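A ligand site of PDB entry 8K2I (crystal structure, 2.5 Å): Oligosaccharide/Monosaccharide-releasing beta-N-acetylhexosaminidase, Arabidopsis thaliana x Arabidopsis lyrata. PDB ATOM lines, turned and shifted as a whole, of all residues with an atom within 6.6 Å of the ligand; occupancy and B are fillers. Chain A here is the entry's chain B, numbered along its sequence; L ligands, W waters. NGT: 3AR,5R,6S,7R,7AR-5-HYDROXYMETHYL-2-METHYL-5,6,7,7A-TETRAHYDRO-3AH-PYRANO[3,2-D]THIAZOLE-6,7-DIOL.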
ATOM      1  N   TYR A 328       3.857  33.476  16.721  1.00  0.00           N
ATOM      2  CA  TYR A 328       4.731  34.623  16.882  1.00  0.00           C
ATOM      3  C   TYR A 328       5.961  34.346  16.021  1.00  0.00           C
ATOM      4  O   TYR A 328       6.518  33.261  16.059  1.00  0.00           O
ATOM      5  CB  TYR A 328       5.097  34.822  18.384  1.00  0.00           C
ATOM      6  CG  TYR A 328       5.884  33.692  19.065  1.00  0.00           C
ATOM      7  CD1 TYR A 328       5.232  32.608  19.651  1.00  0.00           C
ATOM      8  CD2 TYR A 328       7.249  33.703  19.184  1.00  0.00           C
ATOM      9  CE1 TYR A 328       5.913  31.605  20.315  1.00  0.00           C
ATOM     10  CE2 TYR A 328       7.968  32.666  19.791  1.00  0.00           C
ATOM     11  CZ  TYR A 328       7.288  31.597  20.344  1.00  0.00           C
ATOM     12  OH  TYR A 328       7.906  30.512  20.954  1.00  0.00           O
ATOM     13  N   TRP A 332      16.442  34.371  17.210  1.00  0.00           N
ATOM     14  CA  TRP A 332      17.248  34.051  18.385  1.00  0.00           C
ATOM     15  C   TRP A 332      18.524  34.891  18.448  1.00  0.00           C
ATOM     16  O   TRP A 332      19.118  35.228  17.425  1.00  0.00           O
ATOM     17  CB  TRP A 332      17.569  32.558  18.439  1.00  0.00           C
ATOM     18  CG  TRP A 332      16.478  31.675  18.994  1.00  0.00           C
ATOM     19  CD1 TRP A 332      16.228  31.364  20.310  1.00  0.00           C
ATOM     20  CD2 TRP A 332      15.436  31.063  18.199  1.00  0.00           C
ATOM     21  NE1 TRP A 332      15.113  30.566  20.381  1.00  0.00           N
ATOM     22  CE2 TRP A 332      14.595  30.387  19.112  1.00  0.00           C
ATOM     23  CE3 TRP A 332      15.147  31.025  16.844  1.00  0.00           C
ATOM     24  CZ2 TRP A 332      13.468  29.681  18.681  1.00  0.00           C
ATOM     25  CZ3 TRP A 332      14.045  30.308  16.433  1.00  0.00           C
ATOM     26  CH2 TRP A 332      13.205  29.659  17.333  1.00  0.00           C
ATOM     27  N   MET A 336      20.638  33.197  23.761  1.00  0.00           N
ATOM     28  CA  MET A 336      19.248  32.754  23.564  1.00  0.00           C
ATOM     29  C   MET A 336      18.225  33.772  24.087  1.00  0.00           C
ATOM     30  O   MET A 336      17.054  33.420  24.314  1.00  0.00           O
ATOM     31  CB  MET A 336      18.922  31.347  24.134  1.00  0.00           C
ATOM     32  CG  MET A 336      19.877  30.217  23.674  1.00  0.00           C
ATOM     33  SD  MET A 336      19.706  29.803  21.901  1.00  0.00           S
ATOM     34  CE  MET A 336      18.012  29.209  21.914  1.00  0.00           C
ATOM     35  N   TYR A 401       8.092  37.960  25.377  1.00  0.00           N
ATOM     36  CA  TYR A 401       8.894  36.769  25.572  1.00  0.00           C
ATOM     37  C   TYR A 401      10.317  37.149  25.204  1.00  0.00           C
ATOM     38  O   TYR A 401      10.639  37.280  24.004  1.00  0.00           O
ATOM     39  CB  TYR A 401       8.253  35.539  24.861  1.00  0.00           C
ATOM     40  CG  TYR A 401       9.060  34.239  24.826  1.00  0.00           C
ATOM     41  CD1 TYR A 401      10.068  33.961  25.777  1.00  0.00           C
ATOM     42  CD2 TYR A 401       8.918  33.308  23.785  1.00  0.00           C
ATOM     43  CE1 TYR A 401      10.841  32.807  25.726  1.00  0.00           C
ATOM     44  CE2 TYR A 401       9.711  32.158  23.697  1.00  0.00           C
ATOM     45  CZ  TYR A 401      10.642  31.895  24.695  1.00  0.00           C
ATOM     46  OH  TYR A 401      11.404  30.741  24.703  1.00  0.00           O
ATOM     47  N   ASP A 404      14.840  32.669  26.099  1.00  0.00           N
ATOM     48  CA  ASP A 404      14.638  31.259  25.916  1.00  0.00           C
ATOM     49  C   ASP A 404      15.593  30.500  26.827  1.00  0.00           C
ATOM     50  O   ASP A 404      16.775  30.406  26.513  1.00  0.00           O
ATOM     51  CB  ASP A 404      14.798  30.907  24.438  1.00  0.00           C
ATOM     52  CG  ASP A 404      14.503  29.447  24.144  1.00  0.00           C
ATOM     53  OD1 ASP A 404      14.470  28.652  25.140  1.00  0.00           O
ATOM     54  OD2 ASP A 404      14.369  29.094  22.928  1.00  0.00           O
ATOM     55  N   GLU A 405      15.052  29.964  27.943  1.00  0.00           N
ATOM     56  CA  GLU A 405      15.819  29.103  28.823  1.00  0.00           C
ATOM     57  C   GLU A 405      17.084  29.787  29.345  1.00  0.00           C
ATOM     58  O   GLU A 405      18.204  29.449  29.004  1.00  0.00           O
ATOM     59  CB  GLU A 405      16.181  27.774  28.142  1.00  0.00           C
ATOM     60  CG  GLU A 405      14.978  26.942  27.826  1.00  0.00           C
ATOM     61  CD  GLU A 405      15.230  25.587  27.217  1.00  0.00           C
ATOM     62  OE1 GLU A 405      16.253  25.379  26.555  1.00  0.00           O
ATOM     63  OE2 GLU A 405      14.336  24.766  27.375  1.00  0.00           O
ATOM     64  N   THR A 434      10.524  30.990  29.566  1.00  0.00           N
ATOM     65  CA  THR A 434      10.654  29.569  29.400  1.00  0.00           C
ATOM     66  C   THR A 434      11.889  29.116  30.150  1.00  0.00           C
ATOM     67  O   THR A 434      12.970  29.636  29.886  1.00  0.00           O
ATOM     68  CB  THR A 434      10.802  29.137  27.916  1.00  0.00           C
ATOM     69  OG1 THR A 434      11.807  29.903  27.229  1.00  0.00           O
ATOM     70  CG2 THR A 434       9.519  29.195  27.129  1.00  0.00           C
ATOM     71  N   TYR A 435      11.747  28.086  30.987  1.00  0.00           N
ATOM     72  CA  TYR A 435      12.884  27.489  31.676  1.00  0.00           C
ATOM     73  C   TYR A 435      12.685  26.008  31.990  1.00  0.00           C
ATOM     74  O   TYR A 435      11.548  25.526  32.136  1.00  0.00           O
ATOM     75  CB  TYR A 435      13.207  28.286  32.962  1.00  0.00           C
ATOM     76  CG  TYR A 435      12.147  28.302  34.035  1.00  0.00           C
ATOM     77  CD1 TYR A 435      11.069  29.137  33.891  1.00  0.00           C
ATOM     78  CD2 TYR A 435      12.220  27.490  35.175  1.00  0.00           C
ATOM     79  CE1 TYR A 435      10.051  29.157  34.809  1.00  0.00           C
ATOM     80  CE2 TYR A 435      11.156  27.447  36.073  1.00  0.00           C
ATOM     81  CZ  TYR A 435      10.076  28.291  35.885  1.00  0.00           C
ATOM     82  OH  TYR A 435       8.997  28.448  36.735  1.00  0.00           O
ATOM     83  N   CYS A 467       6.679  29.382  32.177  1.00  0.00           N
ATOM     84  CA  CYS A 467       6.469  28.385  31.163  1.00  0.00           C
ATOM     85  C   CYS A 467       7.611  27.382  31.304  1.00  0.00           C
ATOM     86  O   CYS A 467       8.750  27.750  31.054  1.00  0.00           O
ATOM     87  CB  CYS A 467       6.398  29.039  29.797  1.00  0.00           C
ATOM     88  SG  CYS A 467       5.958  27.940  28.398  1.00  0.00           S
ATOM     89  N   TYR A 498       5.739  23.545  28.071  1.00  0.00           N
ATOM     90  CA  TYR A 498       6.194  23.336  26.719  1.00  0.00           C
ATOM     91  C   TYR A 498       6.848  21.974  26.554  1.00  0.00           C
ATOM     92  O   TYR A 498       7.273  21.331  27.539  1.00  0.00           O
ATOM     93  CB  TYR A 498       7.107  24.472  26.280  1.00  0.00           C
ATOM     94  CG  TYR A 498       8.423  24.582  26.976  1.00  0.00           C
ATOM     95  CD1 TYR A 498       9.485  23.859  26.508  1.00  0.00           C
ATOM     96  CD2 TYR A 498       8.601  25.365  28.118  1.00  0.00           C
ATOM     97  CE1 TYR A 498      10.735  23.947  27.121  1.00  0.00           C
ATOM     98  CE2 TYR A 498       9.840  25.460  28.737  1.00  0.00           C
ATOM     99  CZ  TYR A 498      10.911  24.734  28.242  1.00  0.00           C
ATOM    100  OH  TYR A 498      12.174  24.798  28.776  1.00  0.00           O
ATOM    101  N   ILE A 499       6.878  21.538  25.274  1.00  0.00           N
ATOM    102  CA  ILE A 499       7.500  20.274  24.897  1.00  0.00           C
ATOM    103  C   ILE A 499       8.464  20.589  23.777  1.00  0.00           C
ATOM    104  O   ILE A 499       8.164  21.497  23.007  1.00  0.00           O
ATOM    105  CB  ILE A 499       6.504  19.186  24.424  1.00  0.00           C
ATOM    106  CG1 ILE A 499       5.567  19.691  23.312  1.00  0.00           C
ATOM    107  CG2 ILE A 499       5.743  18.552  25.560  1.00  0.00           C
ATOM    108  CD1 ILE A 499       4.797  18.558  22.644  1.00  0.00           C
ATOM    109  N   CYS A 500       9.532  19.763  23.673  1.00  0.00           N
ATOM    110  CA  CYS A 500      10.622  19.987  22.722  1.00  0.00           C
ATOM    111  C   CYS A 500      11.342  18.657  22.438  1.00  0.00           C
ATOM    112  O   CYS A 500      10.701  17.639  22.320  1.00  0.00           O
ATOM    113  CB  CYS A 500      11.544  21.037  23.323  1.00  0.00           C
ATOM    114  SG  CYS A 500      12.118  20.666  24.998  1.00  0.00           S
ATOM    115  N   LEU A 501      12.690  18.617  22.397  1.00  0.00           N
ATOM    116  CA  LEU A 501      13.366  17.343  22.134  1.00  0.00           C
ATOM    117  C   LEU A 501      13.059  16.336  23.241  1.00  0.00           C
ATOM    118  O   LEU A 501      13.203  15.177  22.989  1.00  0.00           O
ATOM    119  CB  LEU A 501      14.874  17.509  21.945  1.00  0.00           C
ATOM    120  CG  LEU A 501      15.759  17.778  23.158  1.00  0.00           C
ATOM    121  CD1 LEU A 501      17.219  17.784  22.757  1.00  0.00           C
ATOM    122  CD2 LEU A 501      15.403  19.130  23.742  1.00  0.00           C
ATOM    123  N   GLY A 502      12.562  16.766  24.396  1.00  0.00           N
ATOM    124  CA  GLY A 502      11.945  15.913  25.371  1.00  0.00           C
ATOM    125  C   GLY A 502      10.556  16.427  25.719  1.00  0.00           C
ATOM    126  O   GLY A 502      10.183  17.543  25.379  1.00  0.00           O
ATOM    127  N   LEU A 535       3.307  26.458  25.003  1.00  0.00           N
ATOM    128  CA  LEU A 535       4.180  27.023  23.985  1.00  0.00           C
ATOM    129  C   LEU A 535       4.927  25.909  23.262  1.00  0.00           C
ATOM    130  O   LEU A 535       5.410  24.986  23.936  1.00  0.00           O
ATOM    131  CB  LEU A 535       5.187  27.931  24.715  1.00  0.00           C
ATOM    132  CG  LEU A 535       6.306  28.588  23.897  1.00  0.00           C
ATOM    133  CD1 LEU A 535       6.653  29.968  24.428  1.00  0.00           C
ATOM    134  CD2 LEU A 535       7.583  27.784  23.903  1.00  0.00           C
ATOM    135  N   TYR A 536       5.002  26.031  21.907  1.00  0.00           N
ATOM    136  CA  TYR A 536       5.903  25.227  21.065  1.00  0.00           C
ATOM    137  C   TYR A 536       6.956  26.130  20.411  1.00  0.00           C
ATOM    138  O   TYR A 536       6.661  27.109  19.741  1.00  0.00           O
ATOM    139  CB  TYR A 536       5.109  24.365  20.031  1.00  0.00           C
ATOM    140  CG  TYR A 536       5.891  23.197  19.474  1.00  0.00           C
ATOM    141  CD1 TYR A 536       6.334  22.154  20.286  1.00  0.00           C
ATOM    142  CD2 TYR A 536       6.224  23.110  18.132  1.00  0.00           C
ATOM    143  CE1 TYR A 536       7.084  21.091  19.792  1.00  0.00           C
ATOM    144  CE2 TYR A 536       6.895  22.010  17.616  1.00  0.00           C
ATOM    145  CZ  TYR A 536       7.379  21.022  18.446  1.00  0.00           C
ATOM    146  OH  TYR A 536       8.097  19.976  17.929  1.00  0.00           O
ATOM    147  N   TRP A 537       8.220  25.775  20.577  1.00  0.00           N
ATOM    148  CA  TRP A 537       9.294  26.690  20.226  1.00  0.00           C
ATOM    149  C   TRP A 537       9.374  27.037  18.731  1.00  0.00           C
ATOM    150  O   TRP A 537       9.981  28.038  18.405  1.00  0.00           O
ATOM    151  CB  TRP A 537      10.609  26.052  20.609  1.00  0.00           C
ATOM    152  CG  TRP A 537      10.986  24.814  19.849  1.00  0.00           C
ATOM    153  CD1 TRP A 537      10.651  23.512  20.130  1.00  0.00           C
ATOM    154  CD2 TRP A 537      12.021  24.742  18.848  1.00  0.00           C
ATOM    155  NE1 TRP A 537      11.352  22.629  19.335  1.00  0.00           N
ATOM    156  CE2 TRP A 537      12.206  23.351  18.549  1.00  0.00           C
ATOM    157  CE3 TRP A 537      12.849  25.701  18.250  1.00  0.00           C
ATOM    158  CZ2 TRP A 537      13.110  22.915  17.574  1.00  0.00           C
ATOM    159  CZ3 TRP A 537      13.746  25.254  17.295  1.00  0.00           C
ATOM    160  CH2 TRP A 537      13.889  23.876  16.960  1.00  0.00           C
ATOM    161  N   ARG A 555      17.252  19.256  11.340  1.00  0.00           N
ATOM    162  CA  ARG A 555      18.412  19.691  12.086  1.00  0.00           C
ATOM    163  C   ARG A 555      19.138  18.527  12.805  1.00  0.00           C
ATOM    164  O   ARG A 555      18.520  17.656  13.421  1.00  0.00           O
ATOM    165  CB  ARG A 555      17.951  20.842  12.996  1.00  0.00           C
ATOM    166  CG  ARG A 555      17.536  22.124  12.243  1.00  0.00           C
ATOM    167  CD  ARG A 555      17.323  23.321  13.158  1.00  0.00           C
ATOM    168  NE  ARG A 555      16.656  24.393  12.470  1.00  0.00           N
ATOM    169  CZ  ARG A 555      16.348  25.572  13.014  1.00  0.00           C
ATOM    170  NH1 ARG A 555      16.647  25.832  14.307  1.00  0.00           N
ATOM    171  NH2 ARG A 555      15.689  26.447  12.233  1.00  0.00           N
ATOM    172  N   LEU A 558      18.654  16.893  16.888  1.00  0.00           N
ATOM    173  CA  LEU A 558      17.301  16.928  17.383  1.00  0.00           C
ATOM    174  C   LEU A 558      16.565  15.720  16.840  1.00  0.00           C
ATOM    175  O   LEU A 558      16.750  15.320  15.694  1.00  0.00           O
ATOM    176  CB  LEU A 558      16.651  18.236  16.909  1.00  0.00           C
ATOM    177  CG  LEU A 558      17.304  19.518  17.405  1.00  0.00           C
ATOM    178  CD1 LEU A 558      16.598  20.738  16.879  1.00  0.00           C
ATOM    179  CD2 LEU A 558      17.296  19.559  18.936  1.00  0.00           C
ATOM    180  N   PRO A 559      15.534  15.204  17.545  1.00  0.00           N
ATOM    181  CA  PRO A 559      14.694  14.149  16.972  1.00  0.00           C
ATOM    182  C   PRO A 559      13.920  14.723  15.749  1.00  0.00           C
ATOM    183  O   PRO A 559      13.145  15.717  15.839  1.00  0.00           O
ATOM    184  CB  PRO A 559      13.805  13.749  18.168  1.00  0.00           C
ATOM    185  CG  PRO A 559      14.509  14.365  19.336  1.00  0.00           C
ATOM    186  CD  PRO A 559      15.015  15.711  18.812  1.00  0.00           C
ATOM    187  N   ASP A 562      10.746  17.396  15.744  1.00  0.00           N
ATOM    188  CA  ASP A 562      10.897  18.457  16.732  1.00  0.00           C
ATOM    189  C   ASP A 562      11.122  19.783  15.977  1.00  0.00           C
ATOM    190  O   ASP A 562      12.037  19.887  15.192  1.00  0.00           O
ATOM    191  CB  ASP A 562      12.022  18.157  17.725  1.00  0.00           C
ATOM    192  CG  ASP A 562      12.171  19.188  18.821  1.00  0.00           C
ATOM    193  OD1 ASP A 562      11.075  19.619  19.425  1.00  0.00           O
ATOM    194  OD2 ASP A 562      13.406  19.534  19.115  1.00  0.00           O
ATOM    195  N   GLY A 563      10.177  20.722  16.121  1.00  0.00           N
ATOM    196  CA  GLY A 563      10.325  22.111  15.673  1.00  0.00           C
ATOM    197  C   GLY A 563       9.727  22.339  14.281  1.00  0.00           C
ATOM    198  O   GLY A 563       9.662  23.447  13.824  1.00  0.00           O
HETATM  199  C1  NGT L   1      13.869  23.833  23.903  1.00  0.00           C
HETATM  200  C2  NGT L   1      14.556  25.199  23.713  1.00  0.00           C
HETATM  201  C3  NGT L   1      14.800  25.554  22.241  1.00  0.00           C
HETATM  202  C4  NGT L   1      15.399  24.387  21.464  1.00  0.00           C
HETATM  203  C5  NGT L   1      14.424  23.218  21.621  1.00  0.00           C
HETATM  204  C6  NGT L   1      14.868  21.988  20.883  1.00  0.00           C
HETATM  205  C7  NGT L   1      12.457  25.910  24.363  1.00  0.00           C
HETATM  206  C8  NGT L   1      11.348  26.787  24.830  1.00  0.00           C
HETATM  207  N2  NGT L   1      13.690  26.212  24.374  1.00  0.00           N
HETATM  208  S1  NGT L   1      12.125  24.336  23.761  1.00  0.00           S
HETATM  209  O3  NGT L   1      15.679  26.671  22.004  1.00  0.00           O
HETATM  210  O4  NGT L   1      15.488  24.725  20.058  1.00  0.00           O
HETATM  211  O5  NGT L   1      14.281  22.823  23.004  1.00  0.00           O
HETATM  212  O6  NGT L   1      14.054  20.875  21.173  1.00  0.00           O
HETATM  213  O   HOH W   1       8.905  24.163  22.824  1.00  0.00           O
HETATM  214  O   HOH W   2      16.077  27.319  19.078  1.00  0.00           O
HETATM  215  O   HOH W   3      11.651  29.106  22.267  1.00  0.00           O
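O6 of the ligand sits at hydrogen-bond distance from OD2 of Asp 562, at 2.5 Å.
A nitrogen (N2) of the ligand is in hydrogen-bond range of the side-chain carboxylate (OD1) of Asp 404 (2.7 Å).
N of Leu 501 lies within hydrogen-bond range of O6 of the ligand (2.9 Å).
The side-chain sulfur of Cys 500 sits close to an oxygen (O5) of the ligand (3.6 Å).
O of Tyr 435 lies close to OH of Tyr 498 (3.5 Å).
The side-chain hydroxyl (OH) of Tyr 498 sits at hydrogen-bond distance from the side-chain carboxylate (OE2) of Glu 405 (2.6 Å).
OD2 of Asp 562 lies within hydrogen-bond range of N of Leu 501 (3.5 Å).
N of Asp 404 lies within hydrogen-bond range of O of Met 336, at 2.9 Å.
The side-chain hydroxyl (OG1) of Thr 434 lies within hydrogen-bond range of the side-chain hydroxyl (OH) of Tyr 401 (2.7 Å).
The side-chain sulfur (SG) of Cys 500 lies close to the backbone carbonyl oxygen (O) of Gly 502 (3.7 Å).
The indole nitrogen (NE1) of Trp 537 lies within hydrogen-bond range of the side-chain carboxylate (OD1) of Asp 562, 3.0 Å away.
OD2 of Asp 404 lies within hydrogen-bond range of NE1 of Trp 332, 3.0 Å away.
The side-chain carboxylate of Glu 405 sits close to a nitrogen (N2) of the ligand (3.4 Å).
Residues that only touch the ligand: Met 336 (3.4 Å), Tyr 401 (3.96 Å), Thr 434 (3.8 Å), Tyr 498 (3.7 Å), Trp 537 (3.3 Å) and Leu 558 (3.9 Å).
Hydrophobic or aromatic side chains that line the ligand: Met 336, Tyr 498, Leu 501, Trp 537 and Leu 558.
11 residues have an atom within 4 Å of the ligand: Met 336, Tyr 401, Asp 404, Glu 405, Thr 434, Tyr 498, Cys 500, Leu 501, Trp 537, Leu 558 and Asp 562.
Water W1 lies within hydrogen-bond range of O of Ile 499 (2.8 Å), N of Trp 537 (2.8 Å) and S1 of the ligand (3.4 Å).
Water W3 lies within hydrogen-bond range of OD2 of Asp 404 (2.8 Å) and OH of Tyr 401 (2.9 Å).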
